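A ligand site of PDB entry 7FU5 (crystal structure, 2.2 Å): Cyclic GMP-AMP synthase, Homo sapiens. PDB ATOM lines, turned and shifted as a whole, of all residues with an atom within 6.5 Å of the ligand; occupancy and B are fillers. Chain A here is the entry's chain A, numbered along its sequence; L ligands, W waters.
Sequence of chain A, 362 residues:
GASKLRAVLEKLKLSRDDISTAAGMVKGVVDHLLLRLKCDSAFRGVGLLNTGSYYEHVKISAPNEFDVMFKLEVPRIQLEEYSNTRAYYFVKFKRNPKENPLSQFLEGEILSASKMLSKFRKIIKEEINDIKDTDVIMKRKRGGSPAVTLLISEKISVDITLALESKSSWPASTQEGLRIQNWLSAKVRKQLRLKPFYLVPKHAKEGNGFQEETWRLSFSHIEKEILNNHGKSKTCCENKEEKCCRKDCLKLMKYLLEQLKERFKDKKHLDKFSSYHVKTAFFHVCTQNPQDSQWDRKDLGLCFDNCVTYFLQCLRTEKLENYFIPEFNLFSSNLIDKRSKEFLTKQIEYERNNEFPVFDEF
O of Ala 87 lies within hydrogen-bond range of N of Leu 217, 3.2 Å away. O of Phe 328 sits at hydrogen-bond distance from N of Asn 322 (2.9 Å). The backbone NH (N) of Phe 324 lies within hydrogen-bond range of the side-chain amide oxygen (OD1) of Asn 322 (2.7 Å). The guanidinium group of Arg 216 lies within hydrogen-bond range of the side-chain hydroxyl of Tyr 88 (3.3 Å). N of Tyr 88 is in hydrogen-bond range of OG1 of Thr 85, at 3.3 Å. The side-chain carboxylate (OE1) of Glu 223 lies within salt-bridge range of the side-chain amino group (NZ) of Lys 279. The backbone carbonyl oxygen of Tyr 276 is in hydrogen-bond range of the side-chain hydroxyl of Thr 280, 2.8 Å away. OG of Ser 274 lies close to N of Tyr 276.
N of Ser 220 sits at hydrogen-bond distance from O1 of the ligand (2.9 Å). N of Phe 219 lies within hydrogen-bond range of N2 of the ligand, 3.0 Å away. O of Leu 217 lies within hydrogen-bond range of N1 of the ligand (2.9 Å). The side-chain amide nitrogen (ND2) of Asn 322 lies within hydrogen-bond range of a nitrogen (N5) of the ligand, at 3.0 Å.
Water W1 lies within hydrogen-bond range of OG of Ser 218 (2.6 Å), O1 of the ligand (2.8 Å), OH of Tyr 276 (3.0 Å) and OG of Ser 220 (3.0 Å).
Residues that only touch the ligand: Ala 87 (3.3 Å), Tyr 88 (3.5 Å), Arg 216 (3.3 Å), Ser 218 (3.6 Å), Glu 223 (3.5 Å), Tyr 276 (3.9 Å), Lys 279 (3.97 Å), Thr 280 (3.9 Å), Phe 283 (3.5 Å), Tyr 323 (3.9 Å), Phe 324 (3.6 Å), Ile 325 (3.4 Å), Phe 328 (3.4 Å) and Leu 330 (3.5 Å). Hydrophobic or aromatic side chains that line the ligand: Ala 87, Phe 219, Tyr 276, Phe 283, Tyr 323, Phe 324, Ile 325, Phe 328 and Leu 330. Of the 28 residues printed, 18 come within 4 Å of the ligand. The nearest printed residue that does not touch the ligand is Leu 335 (4.4 Å).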
ATOM      1  N   THR A  85      10.103   1.671  12.776  1.00  0.00           N
ATOM      2  CA  THR A  85      10.110   0.572  13.743  1.00  0.00           C
ATOM      3  C   THR A  85       8.888  -0.323  13.625  1.00  0.00           C
ATOM      4  O   THR A  85       8.862  -1.385  14.259  1.00  0.00           O
ATOM      5  CB  THR A  85      10.186   1.124  15.172  1.00  0.00           C
ATOM      6  OG1 THR A  85       9.090   2.004  15.407  1.00  0.00           O
ATOM      7  CG2 THR A  85      11.502   1.863  15.390  1.00  0.00           C
ATOM      8  N   ARG A  86       7.881   0.094  12.862  1.00  0.00           N
ATOM      9  CA  ARG A  86       6.694  -0.690  12.516  1.00  0.00           C
ATOM     10  C   ARG A  86       5.757  -0.882  13.698  1.00  0.00           C
ATOM     11  O   ARG A  86       4.616  -1.326  13.520  1.00  0.00           O
ATOM     12  CB  ARG A  86       7.098  -2.067  11.971  1.00  0.00           C
ATOM     13  CG  ARG A  86       7.902  -2.049  10.707  1.00  0.00           C
ATOM     14  CD  ARG A  86       7.011  -1.822   9.499  1.00  0.00           C
ATOM     15  NE  ARG A  86       7.800  -1.642   8.293  1.00  0.00           N
ATOM     16  CZ  ARG A  86       8.376  -0.504   7.943  1.00  0.00           C
ATOM     17  NH1 ARG A  86       8.277   0.582   8.695  1.00  0.00           N
ATOM     18  NH2 ARG A  86       9.083  -0.445   6.815  1.00  0.00           N
ATOM     19  N   ALA A  87       6.202  -0.515  14.895  1.00  0.00           N
ATOM     20  CA  ALA A  87       5.432  -0.786  16.097  1.00  0.00           C
ATOM     21  C   ALA A  87       5.356   0.384  17.059  1.00  0.00           C
ATOM     22  O   ALA A  87       4.425   0.435  17.867  1.00  0.00           O
ATOM     23  CB  ALA A  87       6.018  -1.996  16.851  1.00  0.00           C
ATOM     24  N   TYR A  88       6.291   1.320  16.990  1.00  0.00           N
ATOM     25  CA  TYR A  88       6.304   2.505  17.838  1.00  0.00           C
ATOM     26  C   TYR A  88       5.892   3.710  17.009  1.00  0.00           C
ATOM     27  O   TYR A  88       6.337   3.873  15.869  1.00  0.00           O
ATOM     28  CB  TYR A  88       7.690   2.709  18.462  1.00  0.00           C
ATOM     29  CG  TYR A  88       8.173   1.503  19.249  1.00  0.00           C
ATOM     30  CD1 TYR A  88       8.801   0.441  18.616  1.00  0.00           C
ATOM     31  CD2 TYR A  88       8.006   1.443  20.628  1.00  0.00           C
ATOM     32  CE1 TYR A  88       9.237  -0.657  19.328  1.00  0.00           C
ATOM     33  CE2 TYR A  88       8.448   0.354  21.349  1.00  0.00           C
ATOM     34  CZ  TYR A  88       9.064  -0.696  20.698  1.00  0.00           C
ATOM     35  OH  TYR A  88       9.506  -1.791  21.403  1.00  0.00           O
ATOM     36  N   ARG A 216       3.699   2.075  21.768  1.00  0.00           N
ATOM     37  CA  ARG A 216       3.762   0.801  21.069  1.00  0.00           C
ATOM     38  C   ARG A 216       2.373   0.180  21.005  1.00  0.00           C
ATOM     39  O   ARG A 216       1.586   0.283  21.951  1.00  0.00           O
ATOM     40  CB  ARG A 216       4.735  -0.164  21.757  1.00  0.00           C
ATOM     41  CG  ARG A 216       4.974  -1.452  20.982  1.00  0.00           C
ATOM     42  CD  ARG A 216       6.074  -2.291  21.615  1.00  0.00           C
ATOM     43  NE  ARG A 216       5.631  -2.926  22.855  1.00  0.00           N
ATOM     44  CZ  ARG A 216       6.444  -3.504  23.727  1.00  0.00           C
ATOM     45  NH1 ARG A 216       7.759  -3.520  23.544  1.00  0.00           N
ATOM     46  NH2 ARG A 216       5.933  -4.079  24.809  1.00  0.00           N
ATOM     47  N   LEU A 217       2.091  -0.465  19.873  1.00  0.00           N
ATOM     48  CA  LEU A 217       0.788  -1.095  19.666  1.00  0.00           C
ATOM     49  C   LEU A 217       0.585  -2.261  20.628  1.00  0.00           C
ATOM     50  O   LEU A 217       1.545  -2.915  21.058  1.00  0.00           O
ATOM     51  CB  LEU A 217       0.661  -1.580  18.218  1.00  0.00           C
ATOM     52  CG  LEU A 217       0.633  -0.489  17.150  1.00  0.00           C
ATOM     53  CD1 LEU A 217       0.859  -1.094  15.776  1.00  0.00           C
ATOM     54  CD2 LEU A 217      -0.700   0.233  17.191  1.00  0.00           C
ATOM     55  N   SER A 218      -0.678  -2.529  20.936  1.00  0.00           N
ATOM     56  CA  SER A 218      -1.034  -3.589  21.876  1.00  0.00           C
ATOM     57  C   SER A 218      -2.367  -4.177  21.463  1.00  0.00           C
ATOM     58  O   SER A 218      -3.350  -3.431  21.350  1.00  0.00           O
ATOM     59  CB  SER A 218      -1.089  -3.065  23.313  1.00  0.00           C
ATOM     60  OG  SER A 218      -1.498  -4.083  24.205  1.00  0.00           O
ATOM     61  N   PHE A 219      -2.414  -5.486  21.247  1.00  0.00           N
ATOM     62  CA  PHE A 219      -3.627  -6.197  20.850  1.00  0.00           C
ATOM     63  C   PHE A 219      -4.004  -7.264  21.865  1.00  0.00           C
ATOM     64  O   PHE A 219      -4.396  -8.378  21.511  1.00  0.00           O
ATOM     65  CB  PHE A 219      -3.461  -6.827  19.472  1.00  0.00           C
ATOM     66  CG  PHE A 219      -3.069  -5.855  18.393  1.00  0.00           C
ATOM     67  CD1 PHE A 219      -4.044  -5.155  17.689  1.00  0.00           C
ATOM     68  CD2 PHE A 219      -1.745  -5.638  18.091  1.00  0.00           C
ATOM     69  CE1 PHE A 219      -3.694  -4.265  16.699  1.00  0.00           C
ATOM     70  CE2 PHE A 219      -1.381  -4.743  17.100  1.00  0.00           C
ATOM     71  CZ  PHE A 219      -2.360  -4.056  16.401  1.00  0.00           C
ATOM     72  N   SER A 220      -3.865  -6.935  23.161  1.00  0.00           N
ATOM     73  CA  SER A 220      -4.173  -7.898  24.213  1.00  0.00           C
ATOM     74  C   SER A 220      -5.604  -8.420  24.100  1.00  0.00           C
ATOM     75  O   SER A 220      -5.857  -9.601  24.349  1.00  0.00           O
ATOM     76  CB  SER A 220      -3.967  -7.251  25.587  1.00  0.00           C
ATOM     77  OG  SER A 220      -2.611  -7.327  26.003  1.00  0.00           O
ATOM     78  N   HIS A 221      -6.542  -7.551  23.729  1.00  0.00           N
ATOM     79  CA  HIS A 221      -7.935  -7.970  23.562  1.00  0.00           C
ATOM     80  C   HIS A 221      -8.093  -8.977  22.421  1.00  0.00           C
ATOM     81  O   HIS A 221      -8.957  -9.852  22.494  1.00  0.00           O
ATOM     82  CB  HIS A 221      -8.815  -6.743  23.310  1.00  0.00           C
ATOM     83  CG  HIS A 221      -8.460  -5.990  22.063  1.00  0.00           C
ATOM     84  ND1 HIS A 221      -7.222  -5.408  21.869  1.00  0.00           N
ATOM     85  CD2 HIS A 221      -9.177  -5.730  20.938  1.00  0.00           C
ATOM     86  CE1 HIS A 221      -7.197  -4.826  20.676  1.00  0.00           C
ATOM     87  NE2 HIS A 221      -8.364  -5.005  20.097  1.00  0.00           N
ATOM     88  N   ILE A 222      -7.280  -8.857  21.365  1.00  0.00           N
ATOM     89  CA  ILE A 222      -7.371  -9.804  20.266  1.00  0.00           C
ATOM     90  C   ILE A 222      -6.877 -11.178  20.691  1.00  0.00           C
ATOM     91  O   ILE A 222      -7.500 -12.197  20.384  1.00  0.00           O
ATOM     92  CB  ILE A 222      -6.592  -9.275  19.040  1.00  0.00           C
ATOM     93  CG1 ILE A 222      -7.154  -7.927  18.604  1.00  0.00           C
ATOM     94  CG2 ILE A 222      -6.654 -10.285  17.890  1.00  0.00           C
ATOM     95  CD1 ILE A 222      -8.621  -7.955  18.254  1.00  0.00           C
ATOM     96  N   GLU A 223      -5.748 -11.225  21.411  1.00  0.00           N
ATOM     97  CA  GLU A 223      -5.231 -12.510  21.884  1.00  0.00           C
ATOM     98  C   GLU A 223      -6.214 -13.183  22.826  1.00  0.00           C
ATOM     99  O   GLU A 223      -6.442 -14.396  22.738  1.00  0.00           O
ATOM    100  CB  GLU A 223      -3.891 -12.308  22.581  1.00  0.00           C
ATOM    101  CG  GLU A 223      -3.335 -13.583  23.199  1.00  0.00           C
ATOM    102  CD  GLU A 223      -2.347 -13.321  24.309  1.00  0.00           C
ATOM    103  OE1 GLU A 223      -1.824 -12.200  24.399  1.00  0.00           O
ATOM    104  OE2 GLU A 223      -2.099 -14.260  25.107  1.00  0.00           O
ATOM    105  N   ILE A 226      -9.147 -14.691  20.851  1.00  0.00           N
ATOM    106  CA  ILE A 226      -8.794 -15.887  20.088  1.00  0.00           C
ATOM    107  C   ILE A 226      -8.684 -17.089  21.026  1.00  0.00           C
ATOM    108  O   ILE A 226      -9.192 -18.173  20.721  1.00  0.00           O
ATOM    109  CB  ILE A 226      -7.491 -15.668  19.295  1.00  0.00           C
ATOM    110  CG1 ILE A 226      -7.717 -14.676  18.160  1.00  0.00           C
ATOM    111  CG2 ILE A 226      -6.960 -16.993  18.766  1.00  0.00           C
ATOM    112  CD1 ILE A 226      -6.484 -14.409  17.324  1.00  0.00           C
ATOM    113  N   LYS A 272      15.911 -10.290  28.948  1.00  0.00           N
ATOM    114  CA  LYS A 272      15.330  -9.712  27.750  1.00  0.00           C
ATOM    115  C   LYS A 272      14.105 -10.467  27.240  1.00  0.00           C
ATOM    116  O   LYS A 272      13.359  -9.921  26.430  1.00  0.00           O
ATOM    117  CB  LYS A 272      16.381  -9.660  26.638  1.00  0.00           C
ATOM    118  CG  LYS A 272      17.466  -8.625  26.844  1.00  0.00           C
ATOM    119  CD  LYS A 272      17.032  -7.260  26.325  1.00  0.00           C
ATOM    120  CE  LYS A 272      18.199  -6.300  26.284  1.00  0.00           C
ATOM    121  NZ  LYS A 272      19.352  -6.895  25.544  1.00  0.00           N
ATOM    122  N   SER A 274      10.371 -12.338  27.497  1.00  0.00           N
ATOM    123  CA  SER A 274       9.097 -12.117  28.184  1.00  0.00           C
ATOM    124  C   SER A 274       8.057 -13.062  27.609  1.00  0.00           C
ATOM    125  O   SER A 274       8.311 -13.792  26.642  1.00  0.00           O
ATOM    126  CB  SER A 274       8.649 -10.645  28.050  1.00  0.00           C
ATOM    127  OG  SER A 274       8.382 -10.315  26.707  1.00  0.00           O
ATOM    128  N   SER A 275       6.871 -13.055  28.226  1.00  0.00           N
ATOM    129  CA  SER A 275       5.770 -13.876  27.723  1.00  0.00           C
ATOM    130  C   SER A 275       5.428 -13.548  26.282  1.00  0.00           C
ATOM    131  O   SER A 275       4.895 -14.395  25.561  1.00  0.00           O
ATOM    132  CB  SER A 275       4.542 -13.698  28.628  1.00  0.00           C
ATOM    133  OG  SER A 275       4.257 -12.324  28.826  1.00  0.00           O
ATOM    134  N   TYR A 276       5.746 -12.321  25.834  1.00  0.00           N
ATOM    135  CA  TYR A 276       5.527 -11.942  24.445  1.00  0.00           C
ATOM    136  C   TYR A 276       6.135 -12.957  23.494  1.00  0.00           C
ATOM    137  O   TYR A 276       5.519 -13.319  22.483  1.00  0.00           O
ATOM    138  CB  TYR A 276       6.132 -10.560  24.175  1.00  0.00           C
ATOM    139  CG  TYR A 276       5.187  -9.403  24.382  1.00  0.00           C
ATOM    140  CD1 TYR A 276       4.055  -9.246  23.580  1.00  0.00           C
ATOM    141  CD2 TYR A 276       5.426  -8.443  25.357  1.00  0.00           C
ATOM    142  CE1 TYR A 276       3.186  -8.179  23.758  1.00  0.00           C
ATOM    143  CE2 TYR A 276       4.565  -7.375  25.542  1.00  0.00           C
ATOM    144  CZ  TYR A 276       3.452  -7.255  24.735  1.00  0.00           C
ATOM    145  OH  TYR A 276       2.598  -6.186  24.926  1.00  0.00           O
ATOM    146  N   HIS A 277       7.349 -13.435  23.787  1.00  0.00           N
ATOM    147  CA  HIS A 277       8.074 -14.269  22.842  1.00  0.00           C
ATOM    148  C   HIS A 277       7.440 -15.646  22.711  1.00  0.00           C
ATOM    149  O   HIS A 277       7.251 -16.152  21.600  1.00  0.00           O
ATOM    150  CB  HIS A 277       9.536 -14.374  23.271  1.00  0.00           C
ATOM    151  CG  HIS A 277      10.232 -13.048  23.341  1.00  0.00           C
ATOM    152  ND1 HIS A 277      10.419 -12.370  24.525  1.00  0.00           N
ATOM    153  CD2 HIS A 277      10.764 -12.264  22.368  1.00  0.00           C
ATOM    154  CE1 HIS A 277      11.048 -11.229  24.286  1.00  0.00           C
ATOM    155  NE2 HIS A 277      11.266 -11.145  22.986  1.00  0.00           N
ATOM    156  N   LYS A 279       4.339 -16.486  23.602  1.00  0.00           N
ATOM    157  CA  LYS A 279       3.003 -16.296  23.042  1.00  0.00           C
ATOM    158  C   LYS A 279       3.055 -16.140  21.529  1.00  0.00           C
ATOM    159  O   LYS A 279       2.224 -16.689  20.800  1.00  0.00           O
ATOM    160  CB  LYS A 279       2.330 -15.078  23.692  1.00  0.00           C
ATOM    161  CG  LYS A 279       1.644 -15.373  25.015  1.00  0.00           C
ATOM    162  CD  LYS A 279       1.890 -14.291  26.057  1.00  0.00           C
ATOM    163  CE  LYS A 279       0.676 -13.395  26.278  1.00  0.00           C
ATOM    164  NZ  LYS A 279       0.465 -12.419  25.173  1.00  0.00           N
ATOM    165  N   THR A 280       4.054 -15.392  21.032  1.00  0.00           N
ATOM    166  CA  THR A 280       4.195 -15.191  19.597  1.00  0.00           C
ATOM    167  C   THR A 280       4.545 -16.487  18.876  1.00  0.00           C
ATOM    168  O   THR A 280       4.008 -16.762  17.792  1.00  0.00           O
ATOM    169  CB  THR A 280       5.259 -14.120  19.342  1.00  0.00           C
ATOM    170  OG1 THR A 280       4.805 -12.862  19.842  1.00  0.00           O
ATOM    171  CG2 THR A 280       5.537 -13.995  17.851  1.00  0.00           C
ATOM    172  N   PHE A 283       1.335 -18.836  18.652  1.00  0.00           N
ATOM    173  CA  PHE A 283       0.350 -18.460  17.653  1.00  0.00           C
ATOM    174  C   PHE A 283       0.845 -18.739  16.230  1.00  0.00           C
ATOM    175  O   PHE A 283       0.037 -19.018  15.345  1.00  0.00           O
ATOM    176  CB  PHE A 283      -0.022 -16.980  17.812  1.00  0.00           C
ATOM    177  CG  PHE A 283      -1.107 -16.751  18.824  1.00  0.00           C
ATOM    178  CD1 PHE A 283      -2.437 -16.770  18.460  1.00  0.00           C
ATOM    179  CD2 PHE A 283      -0.787 -16.523  20.153  1.00  0.00           C
ATOM    180  CE1 PHE A 283      -3.435 -16.559  19.394  1.00  0.00           C
ATOM    181  CE2 PHE A 283      -1.777 -16.311  21.093  1.00  0.00           C
ATOM    182  CZ  PHE A 283      -3.107 -16.336  20.713  1.00  0.00           C
ATOM    183  N   ASN A 322       6.606 -10.796  14.800  1.00  0.00           N
ATOM    184  CA  ASN A 322       5.421 -10.448  15.577  1.00  0.00           C
ATOM    185  C   ASN A 322       4.173 -10.942  14.857  1.00  0.00           C
ATOM    186  O   ASN A 322       4.075 -10.893  13.637  1.00  0.00           O
ATOM    187  CB  ASN A 322       5.358  -8.928  15.777  1.00  0.00           C
ATOM    188  CG  ASN A 322       4.108  -8.501  16.519  1.00  0.00           C
ATOM    189  OD1 ASN A 322       3.060  -8.294  15.916  1.00  0.00           O
ATOM    190  ND2 ASN A 322       4.219  -8.368  17.829  1.00  0.00           N
ATOM    191  N   TYR A 323       3.217 -11.452  15.644  1.00  0.00           N
ATOM    192  CA  TYR A 323       2.051 -12.087  15.037  1.00  0.00           C
ATOM    193  C   TYR A 323       1.178 -11.075  14.286  1.00  0.00           C
ATOM    194  O   TYR A 323       0.496 -11.449  13.326  1.00  0.00           O
ATOM    195  CB  TYR A 323       1.227 -12.807  16.103  1.00  0.00           C
ATOM    196  CG  TYR A 323       0.291 -13.848  15.547  1.00  0.00           C
ATOM    197  CD1 TYR A 323       0.780 -15.002  14.950  1.00  0.00           C
ATOM    198  CD2 TYR A 323      -1.089 -13.674  15.610  1.00  0.00           C
ATOM    199  CE1 TYR A 323      -0.075 -15.956  14.432  1.00  0.00           C
ATOM    200  CE2 TYR A 323      -1.952 -14.622  15.102  1.00  0.00           C
ATOM    201  CZ  TYR A 323      -1.437 -15.763  14.519  1.00  0.00           C
ATOM    202  OH  TYR A 323      -2.281 -16.726  14.005  1.00  0.00           O
ATOM    203  N   PHE A 324       1.191  -9.817  14.709  1.00  0.00           N
ATOM    204  CA  PHE A 324       0.393  -8.776  14.071  1.00  0.00           C
ATOM    205  C   PHE A 324       1.199  -7.877  13.150  1.00  0.00           C
ATOM    206  O   PHE A 324       0.636  -7.315  12.203  1.00  0.00           O
ATOM    207  CB  PHE A 324      -0.297  -7.902  15.132  1.00  0.00           C
ATOM    208  CG  PHE A 324      -1.160  -8.675  16.088  1.00  0.00           C
ATOM    209  CD1 PHE A 324      -0.624  -9.211  17.245  1.00  0.00           C
ATOM    210  CD2 PHE A 324      -2.507  -8.851  15.835  1.00  0.00           C
ATOM    211  CE1 PHE A 324      -1.422  -9.924  18.132  1.00  0.00           C
ATOM    212  CE2 PHE A 324      -3.310  -9.551  16.710  1.00  0.00           C
ATOM    213  CZ  PHE A 324      -2.758 -10.092  17.864  1.00  0.00           C
ATOM    214  N   ILE A 325       2.492  -7.718  13.407  1.00  0.00           N
ATOM    215  CA  ILE A 325       3.352  -6.842  12.611  1.00  0.00           C
ATOM    216  C   ILE A 325       4.494  -7.691  12.060  1.00  0.00           C
ATOM    217  O   ILE A 325       5.566  -7.753  12.674  1.00  0.00           O
ATOM    218  CB  ILE A 325       3.858  -5.654  13.431  1.00  0.00           C
ATOM    219  CG1 ILE A 325       2.688  -4.958  14.141  1.00  0.00           C
ATOM    220  CG2 ILE A 325       4.593  -4.657  12.546  1.00  0.00           C
ATOM    221  CD1 ILE A 325       3.107  -3.881  15.109  1.00  0.00           C
ATOM    222  N   PHE A 328       8.309  -6.925  12.141  1.00  0.00           N
ATOM    223  CA  PHE A 328       8.964  -6.741  13.419  1.00  0.00           C
ATOM    224  C   PHE A 328       9.520  -8.087  13.878  1.00  0.00           C
ATOM    225  O   PHE A 328       8.765  -9.038  14.091  1.00  0.00           O
ATOM    226  CB  PHE A 328       8.001  -6.172  14.454  1.00  0.00           C
ATOM    227  CG  PHE A 328       8.677  -5.543  15.635  1.00  0.00           C
ATOM    228  CD1 PHE A 328       9.200  -6.322  16.658  1.00  0.00           C
ATOM    229  CD2 PHE A 328       8.796  -4.165  15.724  1.00  0.00           C
ATOM    230  CE1 PHE A 328       9.829  -5.740  17.739  1.00  0.00           C
ATOM    231  CE2 PHE A 328       9.420  -3.587  16.812  1.00  0.00           C
ATOM    232  CZ  PHE A 328       9.935  -4.372  17.812  1.00  0.00           C
ATOM    233  N   LEU A 330      11.158  -9.934  16.707  1.00  0.00           N
ATOM    234  CA  LEU A 330      11.416  -9.884  18.141  1.00  0.00           C
ATOM    235  C   LEU A 330      12.761 -10.480  18.515  1.00  0.00           C
ATOM    236  O   LEU A 330      13.265 -10.216  19.608  1.00  0.00           O
ATOM    237  CB  LEU A 330      10.308 -10.613  18.904  1.00  0.00           C
ATOM    238  CG  LEU A 330       8.882 -10.077  18.764  1.00  0.00           C
ATOM    239  CD1 LEU A 330       7.894 -11.044  19.388  1.00  0.00           C
ATOM    240  CD2 LEU A 330       8.749  -8.692  19.384  1.00  0.00           C
ATOM    241  N   LEU A 335      17.721  -6.400  19.213  1.00  0.00           N
ATOM    242  CA  LEU A 335      16.795  -6.548  20.331  1.00  0.00           C
ATOM    243  C   LEU A 335      17.311  -7.541  21.375  1.00  0.00           C
ATOM    244  O   LEU A 335      17.300  -7.234  22.571  1.00  0.00           O
ATOM    245  CB  LEU A 335      15.420  -6.977  19.818  1.00  0.00           C
ATOM    246  CG  LEU A 335      14.644  -5.856  19.116  1.00  0.00           C
ATOM    247  CD1 LEU A 335      13.467  -6.400  18.342  1.00  0.00           C
ATOM    248  CD2 LEU A 335      14.194  -4.830  20.139  1.00  0.00           C
HETATM  249  C1  LIG L   1       9.074  -6.996  23.127  1.00  0.00           C
HETATM  250  C2  LIG L   1      10.194  -6.295  22.754  1.00  0.00           C
HETATM  251  C3  LIG L   1       8.927  -5.245  21.013  1.00  0.00           C
HETATM  252  C4  LIG L   1       1.266  -6.601  19.990  1.00  0.00           C
HETATM  253  C5  LIG L   1      -0.516  -8.845  21.910  1.00  0.00           C
HETATM  254  C6  LIG L   1      -0.226 -10.248  21.918  1.00  0.00           C
HETATM  255  C7  LIG L   1       0.778 -10.794  21.170  1.00  0.00           C
HETATM  256  C8  LIG L   1       1.323  -8.640  20.324  1.00  0.00           C
HETATM  257  C9  LIG L   1       1.124 -12.251  21.125  1.00  0.00           C
HETATM  258  C10 LIG L   1       0.494 -13.028  19.973  1.00  0.00           C
HETATM  259  C11 LIG L   1      -1.017 -13.020  20.000  1.00  0.00           C
HETATM  260  C12 LIG L   1      10.118  -5.413  21.691  1.00  0.00           C
HETATM  261  C13 LIG L   1       2.760  -5.265  18.529  1.00  0.00           C
HETATM  262  C14 LIG L   1       5.287  -5.409  18.625  1.00  0.00           C
HETATM  263  C15 LIG L   1       4.070  -5.440  19.267  1.00  0.00           C
HETATM  264  C16 LIG L   1       4.101  -5.640  20.644  1.00  0.00           C
HETATM  265  C17 LIG L   1       5.284  -5.809  21.317  1.00  0.00           C
HETATM  266  C18 LIG L   1       6.505  -5.771  20.654  1.00  0.00           C
HETATM  267  C19 LIG L   1       6.487  -5.566  19.276  1.00  0.00           C
HETATM  268  C20 LIG L   1       7.785  -5.950  21.381  1.00  0.00           C
HETATM  269  C21 LIG L   1       7.882  -6.828  22.449  1.00  0.00           C
HETATM  270  F1  LIG L   1       5.286  -5.201  17.289  1.00  0.00           F
HETATM  271  N1  LIG L   1       1.637  -5.378  19.459  1.00  0.00           N
HETATM  272  N2  LIG L   1       0.275  -6.749  20.868  1.00  0.00           N
HETATM  273  N3  LIG L   1       0.332  -8.112  21.072  1.00  0.00           N
HETATM  274  N4  LIG L   1       1.546  -9.984  20.365  1.00  0.00           N
HETATM  275  N5  LIG L   1       1.952  -7.729  19.627  1.00  0.00           N
HETATM  276  O1  LIG L   1      -1.393  -8.278  22.561  1.00  0.00           O
HETATM  277  O   HOH W   1      -0.289  -6.383  24.269  1.00  0.00           O
HETATM  278  O   HOH W   2       3.373 -11.502  18.392  1.00  0.00           O
